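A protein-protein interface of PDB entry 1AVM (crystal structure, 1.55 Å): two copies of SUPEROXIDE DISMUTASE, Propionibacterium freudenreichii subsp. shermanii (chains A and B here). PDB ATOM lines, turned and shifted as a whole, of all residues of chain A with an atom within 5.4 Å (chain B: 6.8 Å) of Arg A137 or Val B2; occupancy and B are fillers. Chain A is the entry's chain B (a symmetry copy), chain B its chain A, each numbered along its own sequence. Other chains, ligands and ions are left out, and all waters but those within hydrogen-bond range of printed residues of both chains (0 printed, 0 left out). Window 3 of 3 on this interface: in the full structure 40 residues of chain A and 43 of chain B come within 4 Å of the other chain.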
ATOM      1  N   PHE A 103     -12.231 -16.181   1.779  1.00  0.00           N
ATOM      2  CA  PHE A 103     -12.670 -15.539   3.013  1.00  0.00           C
ATOM      3  C   PHE A 103     -14.141 -15.695   3.388  1.00  0.00           C
ATOM      4  O   PHE A 103     -14.524 -15.383   4.516  1.00  0.00           O
ATOM      5  CB  PHE A 103     -12.281 -14.058   2.995  1.00  0.00           C
ATOM      6  CG  PHE A 103     -10.807 -13.828   2.813  1.00  0.00           C
ATOM      7  CD1 PHE A 103      -9.891 -14.345   3.727  1.00  0.00           C
ATOM      8  CD2 PHE A 103     -10.331 -13.128   1.710  1.00  0.00           C
ATOM      9  CE1 PHE A 103      -8.523 -14.173   3.540  1.00  0.00           C
ATOM     10  CE2 PHE A 103      -8.965 -12.951   1.512  1.00  0.00           C
ATOM     11  CZ  PHE A 103      -8.059 -13.474   2.428  1.00  0.00           C
ATOM     12  N   VAL A 130     -14.523  -4.686   2.994  1.00  0.00           N
ATOM     13  CA  VAL A 130     -13.236  -4.009   3.102  1.00  0.00           C
ATOM     14  C   VAL A 130     -12.033  -4.933   3.127  1.00  0.00           C
ATOM     15  O   VAL A 130     -12.148  -6.128   3.404  1.00  0.00           O
ATOM     16  CB  VAL A 130     -13.153  -3.154   4.399  1.00  0.00           C
ATOM     17  CG1 VAL A 130     -14.230  -2.081   4.413  1.00  0.00           C
ATOM     18  CG2 VAL A 130     -13.274  -4.050   5.629  1.00  0.00           C
ATOM     19  N   TRP A 131     -10.875  -4.359   2.823  1.00  0.00           N
ATOM     20  CA  TRP A 131      -9.624  -5.086   2.874  1.00  0.00           C
ATOM     21  C   TRP A 131      -9.013  -4.716   4.221  1.00  0.00           C
ATOM     22  O   TRP A 131      -8.869  -3.536   4.554  1.00  0.00           O
ATOM     23  CB  TRP A 131      -8.679  -4.666   1.743  1.00  0.00           C
ATOM     24  CG  TRP A 131      -7.298  -5.252   1.887  1.00  0.00           C
ATOM     25  CD1 TRP A 131      -6.152  -4.584   2.228  1.00  0.00           C
ATOM     26  CD2 TRP A 131      -6.926  -6.627   1.727  1.00  0.00           C
ATOM     27  NE1 TRP A 131      -5.095  -5.459   2.293  1.00  0.00           N
ATOM     28  CE2 TRP A 131      -5.540  -6.719   1.990  1.00  0.00           C
ATOM     29  CE3 TRP A 131      -7.630  -7.792   1.388  1.00  0.00           C
ATOM     30  CZ2 TRP A 131      -4.844  -7.929   1.924  1.00  0.00           C
ATOM     31  CZ3 TRP A 131      -6.936  -8.995   1.321  1.00  0.00           C
ATOM     32  CH2 TRP A 131      -5.556  -9.052   1.589  1.00  0.00           C
ATOM     33  N   ASP A 132      -8.724  -5.741   5.010  1.00  0.00           N
ATOM     34  CA  ASP A 132      -8.117  -5.609   6.327  1.00  0.00           C
ATOM     35  C   ASP A 132      -6.615  -5.817   6.124  1.00  0.00           C
ATOM     36  O   ASP A 132      -6.171  -6.935   5.883  1.00  0.00           O
ATOM     37  CB  ASP A 132      -8.709  -6.688   7.248  1.00  0.00           C
ATOM     38  CG  ASP A 132      -7.947  -6.854   8.554  1.00  0.00           C
ATOM     39  OD1 ASP A 132      -7.221  -5.932   8.979  1.00  0.00           O
ATOM     40  OD2 ASP A 132      -8.090  -7.936   9.162  1.00  0.00           O
ATOM     41  N   PRO A 133      -5.820  -4.735   6.219  1.00  0.00           N
ATOM     42  CA  PRO A 133      -4.361  -4.758   6.046  1.00  0.00           C
ATOM     43  C   PRO A 133      -3.621  -5.558   7.113  1.00  0.00           C
ATOM     44  O   PRO A 133      -2.595  -6.178   6.834  1.00  0.00           O
ATOM     45  CB  PRO A 133      -3.980  -3.276   6.142  1.00  0.00           C
ATOM     46  CG  PRO A 133      -5.250  -2.546   5.831  1.00  0.00           C
ATOM     47  CD  PRO A 133      -6.279  -3.373   6.530  1.00  0.00           C
ATOM     48  N   GLY A 135      -4.929  -8.155   9.127  1.00  0.00           N
ATOM     49  CA  GLY A 135      -5.199  -9.574   8.997  1.00  0.00           C
ATOM     50  C   GLY A 135      -5.049 -10.074   7.571  1.00  0.00           C
ATOM     51  O   GLY A 135      -5.123 -11.280   7.330  1.00  0.00           O
ATOM     52  N   LYS A 136      -4.832  -9.149   6.635  1.00  0.00           N
ATOM     53  CA  LYS A 136      -4.676  -9.464   5.213  1.00  0.00           C
ATOM     54  C   LYS A 136      -5.824 -10.331   4.714  1.00  0.00           C
ATOM     55  O   LYS A 136      -5.619 -11.411   4.163  1.00  0.00           O
ATOM     56  CB  LYS A 136      -3.325 -10.133   4.948  1.00  0.00           C
ATOM     57  CG  LYS A 136      -2.146  -9.190   5.131  1.00  0.00           C
ATOM     58  CD  LYS A 136      -0.839  -9.832   4.701  1.00  0.00           C
ATOM     59  CE  LYS A 136       0.299  -8.823   4.740  1.00  0.00           C
ATOM     60  NZ  LYS A 136       1.601  -9.427   4.333  1.00  0.00           N
ATOM     61  N   ARG A 137      -7.038  -9.821   4.892  1.00  0.00           N
ATOM     62  CA  ARG A 137      -8.242 -10.538   4.501  1.00  0.00           C
ATOM     63  C   ARG A 137      -9.363  -9.572   4.143  1.00  0.00           C
ATOM     64  O   ARG A 137      -9.255  -8.371   4.371  1.00  0.00           O
ATOM     65  CB  ARG A 137      -8.705 -11.424   5.660  1.00  0.00           C
ATOM     66  CG  ARG A 137      -9.005 -10.652   6.945  1.00  0.00           C
ATOM     67  CD  ARG A 137      -9.442 -11.578   8.068  1.00  0.00           C
ATOM     68  NE  ARG A 137     -10.664 -12.307   7.731  1.00  0.00           N
ATOM     69  CZ  ARG A 137     -10.747 -13.627   7.594  1.00  0.00           C
ATOM     70  NH1 ARG A 137      -9.677 -14.390   7.761  1.00  0.00           N
ATOM     71  NH2 ARG A 137     -11.910 -14.185   7.287  1.00  0.00           N
ATOM     72  N   ILE A 138     -10.427 -10.108   3.560  1.00  0.00           N
ATOM     73  CA  ILE A 138     -11.586  -9.307   3.199  1.00  0.00           C
ATOM     74  C   ILE A 138     -12.639  -9.576   4.267  1.00  0.00           C
ATOM     75  O   ILE A 138     -12.942 -10.731   4.565  1.00  0.00           O
ATOM     76  CB  ILE A 138     -12.158  -9.706   1.818  1.00  0.00           C
ATOM     77  CG1 ILE A 138     -11.121  -9.460   0.721  1.00  0.00           C
ATOM     78  CG2 ILE A 138     -13.434  -8.919   1.531  1.00  0.00           C
ATOM     79  CD1 ILE A 138     -11.596  -9.852  -0.672  1.00  0.00           C
ATOM     80  N   ASN A 139     -13.157  -8.507   4.866  1.00  0.00           N
ATOM     81  CA  ASN A 139     -14.179  -8.605   5.904  1.00  0.00           C
ATOM     82  C   ASN A 139     -15.378  -7.750   5.530  1.00  0.00           C
ATOM     83  O   ASN A 139     -15.293  -6.904   4.642  1.00  0.00           O
ATOM     84  CB  ASN A 139     -13.654  -8.053   7.240  1.00  0.00           C
ATOM     85  CG  ASN A 139     -12.562  -8.906   7.862  1.00  0.00           C
ATOM     86  OD1 ASN A 139     -11.689  -8.390   8.558  1.00  0.00           O
ATOM     87  ND2 ASN A 139     -12.624 -10.211   7.651  1.00  0.00           N
ATOM     88  N   ALA B   1      -4.012 -18.566  14.612  1.00  0.00           N
ATOM     89  CA  ALA B   1      -5.127 -17.580  14.655  1.00  0.00           C
ATOM     90  C   ALA B   1      -4.902 -16.501  13.607  1.00  0.00           C
ATOM     91  O   ALA B   1      -3.788 -16.335  13.107  1.00  0.00           O
ATOM     92  CB  ALA B   1      -5.222 -16.956  16.042  1.00  0.00           C
ATOM     93  N   VAL B   2      -5.962 -15.772  13.271  1.00  0.00           N
ATOM     94  CA  VAL B   2      -5.863 -14.703  12.285  1.00  0.00           C
ATOM     95  C   VAL B   2      -5.086 -13.533  12.877  1.00  0.00           C
ATOM     96  O   VAL B   2      -4.162 -13.010  12.255  1.00  0.00           O
ATOM     97  CB  VAL B   2      -7.260 -14.226  11.824  1.00  0.00           C
ATOM     98  CG1 VAL B   2      -7.136 -13.028  10.890  1.00  0.00           C
ATOM     99  CG2 VAL B   2      -7.986 -15.360  11.119  1.00  0.00           C
ATOM    100  N   TYR B   3      -5.453 -13.148  14.095  1.00  0.00           N
ATOM    101  CA  TYR B   3      -4.798 -12.044  14.782  1.00  0.00           C
ATOM    102  C   TYR B   3      -3.937 -12.545  15.927  1.00  0.00           C
ATOM    103  O   TYR B   3      -4.298 -13.488  16.632  1.00  0.00           O
ATOM    104  CB  TYR B   3      -5.837 -11.049  15.303  1.00  0.00           C
ATOM    105  CG  TYR B   3      -6.736 -10.513  14.218  1.00  0.00           C
ATOM    106  CD1 TYR B   3      -6.232  -9.691  13.212  1.00  0.00           C
ATOM    107  CD2 TYR B   3      -8.088 -10.853  14.181  1.00  0.00           C
ATOM    108  CE1 TYR B   3      -7.049  -9.222  12.190  1.00  0.00           C
ATOM    109  CE2 TYR B   3      -8.916 -10.389  13.167  1.00  0.00           C
ATOM    110  CZ  TYR B   3      -8.392  -9.577  12.173  1.00  0.00           C
ATOM    111  OH  TYR B   3      -9.207  -9.128  11.160  1.00  0.00           O
ATOM    112  N   THR B   4      -2.791 -11.899  16.106  1.00  0.00           N
ATOM    113  CA  THR B   4      -1.857 -12.263  17.162  1.00  0.00           C
ATOM    114  C   THR B   4      -1.414 -11.028  17.934  1.00  0.00           C
ATOM    115  O   THR B   4      -1.401  -9.919  17.399  1.00  0.00           O
ATOM    116  CB  THR B   4      -0.606 -12.983  16.592  1.00  0.00           C
ATOM    117  OG1 THR B   4       0.028 -12.152  15.613  1.00  0.00           O
ATOM    118  CG2 THR B   4      -0.996 -14.303  15.948  1.00  0.00           C
ATOM    119  N   VAL B  36      -7.382  -8.923  20.868  1.00  0.00           N
ATOM    120  CA  VAL B  36      -6.938  -9.904  19.884  1.00  0.00           C
ATOM    121  C   VAL B  36      -7.859 -11.121  19.963  1.00  0.00           C
ATOM    122  O   VAL B  36      -8.352 -11.599  18.942  1.00  0.00           O
ATOM    123  CB  VAL B  36      -5.474 -10.332  20.136  1.00  0.00           C
ATOM    124  CG1 VAL B  36      -5.088 -11.466  19.205  1.00  0.00           C
ATOM    125  CG2 VAL B  36      -4.542  -9.145  19.939  1.00  0.00           C
ATOM    126  N   ALA B  39     -11.291 -10.209  18.604  1.00  0.00           N
ATOM    127  CA  ALA B  39     -11.317 -10.083  17.148  1.00  0.00           C
ATOM    128  C   ALA B  39     -11.347 -11.462  16.489  1.00  0.00           C
ATOM    129  O   ALA B  39     -12.050 -11.670  15.500  1.00  0.00           O
ATOM    130  CB  ALA B  39     -10.114  -9.286  16.664  1.00  0.00           C
ATOM    131  N   ASN B  40     -10.582 -12.400  17.044  1.00  0.00           N
ATOM    132  CA  ASN B  40     -10.538 -13.762  16.518  1.00  0.00           C
ATOM    133  C   ASN B  40     -11.878 -14.453  16.708  1.00  0.00           C
ATOM    134  O   ASN B  40     -12.369 -15.132  15.807  1.00  0.00           O
ATOM    135  CB  ASN B  40      -9.449 -14.576  17.219  1.00  0.00           C
ATOM    136  CG  ASN B  40      -8.070 -14.281  16.681  1.00  0.00           C
ATOM    137  OD1 ASN B  40      -7.894 -14.059  15.485  1.00  0.00           O
ATOM    138  ND2 ASN B  40      -7.078 -14.289  17.559  1.00  0.00           N
ATOM    139  N   LEU B  43     -14.584 -13.319  14.222  1.00  0.00           N
ATOM    140  CA  LEU B  43     -14.412 -13.946  12.913  1.00  0.00           C
ATOM    141  C   LEU B  43     -14.919 -15.387  12.910  1.00  0.00           C
ATOM    142  O   LEU B  43     -15.520 -15.833  11.931  1.00  0.00           O
ATOM    143  CB  LEU B  43     -12.946 -13.909  12.476  1.00  0.00           C
ATOM    144  CG  LEU B  43     -12.372 -12.561  12.036  1.00  0.00           C
ATOM    145  CD1 LEU B  43     -10.935 -12.761  11.583  1.00  0.00           C
ATOM    146  CD2 LEU B  43     -13.207 -11.977  10.906  1.00  0.00           C
ATOM    147  N   ASP B  44     -14.669 -16.109  14.002  1.00  0.00           N
ATOM    148  CA  ASP B  44     -15.119 -17.496  14.130  1.00  0.00           C
ATOM    149  C   ASP B  44     -16.645 -17.591  14.139  1.00  0.00           C
ATOM    150  O   ASP B  44     -17.222 -18.469  13.499  1.00  0.00           O
ATOM    151  CB  ASP B  44     -14.566 -18.131  15.412  1.00  0.00           C
ATOM    152  CG  ASP B  44     -13.077 -18.426  15.331  1.00  0.00           C
ATOM    153  OD1 ASP B  44     -12.556 -18.623  14.209  1.00  0.00           O
ATOM    154  OD2 ASP B  44     -12.427 -18.475  16.397  1.00  0.00           O
ATOM    155  N   ARG B  50     -22.237 -18.029   8.565  1.00  0.00           N
ATOM    156  CA  ARG B  50     -22.316 -18.328   7.138  1.00  0.00           C
ATOM    157  C   ARG B  50     -22.591 -19.810   6.906  1.00  0.00           C
ATOM    158  O   ARG B  50     -23.401 -20.164   6.052  1.00  0.00           O
ATOM    159  CB  ARG B  50     -21.025 -17.935   6.414  1.00  0.00           C
ATOM    160  CG  ARG B  50     -20.790 -16.438   6.285  1.00  0.00           C
ATOM    161  CD  ARG B  50     -19.597 -16.135   5.386  1.00  0.00           C
ATOM    162  NE  ARG B  50     -18.360 -16.738   5.873  1.00  0.00           N
ATOM    163  CZ  ARG B  50     -17.530 -16.159   6.735  1.00  0.00           C
ATOM    164  NH1 ARG B  50     -17.787 -14.950   7.217  1.00  0.00           N
ATOM    165  NH2 ARG B  50     -16.448 -16.804   7.140  1.00  0.00           N
ATOM    166  N   HIS B  72      -7.291  -3.650  18.497  1.00  0.00           N
ATOM    167  CA  HIS B  72      -6.048  -4.334  18.152  1.00  0.00           C
ATOM    168  C   HIS B  72      -5.181  -3.436  17.265  1.00  0.00           C
ATOM    169  O   HIS B  72      -3.989  -3.275  17.512  1.00  0.00           O
ATOM    170  CB  HIS B  72      -6.364  -5.658  17.442  1.00  0.00           C
ATOM    171  CG  HIS B  72      -5.154  -6.424  17.006  1.00  0.00           C
ATOM    172  ND1 HIS B  72      -5.167  -7.280  15.924  1.00  0.00           N
ATOM    173  CD2 HIS B  72      -3.893  -6.464  17.497  1.00  0.00           C
ATOM    174  CE1 HIS B  72      -3.967  -7.813  15.769  1.00  0.00           C
ATOM    175  NE2 HIS B  72      -3.175  -7.332  16.711  1.00  0.00           N
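No position is printed for both chains. Of the 8 pairs that touch across the chains among the printed residues, none has its exchanged pair printed and touching as well.
Among the printed residues, pairs that only touch across the chains: Phe A103 with Arg B50 (3.6 Å), Asn A139 with Tyr B3 (3.7 Å), Gly A135 with Tyr B3 (3.7 Å), Asn A139 with Leu B43 (3.7 Å), Arg A137 with Val B2 (3.9 Å), Arg A137 with Leu B43 (3.9 Å) and Arg A137 with Tyr B3 (3.95 Å).
The backbone NH (N) of Val B2 is in hydrogen-bond range of the side-chain amide oxygen (OD1) of Asn B40 (3.4 Å). The backbone NH (N) of Tyr B3 lies within hydrogen-bond range of the side-chain amide oxygen (OD1) of Asn B40, 3.0 Å away. The backbone carbonyl oxygen (O) of Asn A139 lies within hydrogen-bond range of the backbone NH (N) of Val A130. The backbone NH (N) of Gly A135 sits at hydrogen-bond distance from the side-chain carboxylate (OD2) of Asp A132, 3.2 Å away. The backbone NH (N) of Asp A132 lies within hydrogen-bond range of the backbone carbonyl oxygen (O) of Arg A137 (2.8 Å). NE of Arg A137 sits close to ND2 of Asn A139 (2.9 Å).
The side-chain carboxylate of Asp A132 lies within hydrogen-bond range of the side-chain hydroxyl of Tyr B3 (2.6 Å).
Of the printed residues of chain B, Asp A132 touches Tyr B3 (2.6 Å). Of the printed residues of chain B, Gly A135 touches Tyr B3. Of chain B, only Val B2 (3.9 Å), Tyr B3 (3.95 Å) and Leu B43 (3.9 Å) come within 4 Å of Arg A137. Printed residues of chain A within 4 Å of Val B2: Arg A137 (3.9 Å). Ala B39 touches none of the printed residues of chain A. The nearest residue of chain A that does not touch Val B2 is Gly A135 (4.4 Å).
Of the 11 printed residues of chain B, 4 touch a printed residue of chain A. Printed residues of chain B that touch a printed residue of chain A: Val B2, Tyr B3, Leu B43 and Arg B50. Hydrophobic or aromatic side chains of chain B that line the printed part of chain A: Val B2, Tyr B3 and Leu B43. Of the 10 printed residues of chain A, 5 touch a printed residue of chain B. Among the printed residues, 8 pairs touch across the chains. Among the printed residues, no Asp or Glu carboxylate lies within 4 Å of a Lys or Arg side-chain nitrogen of the other chain.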
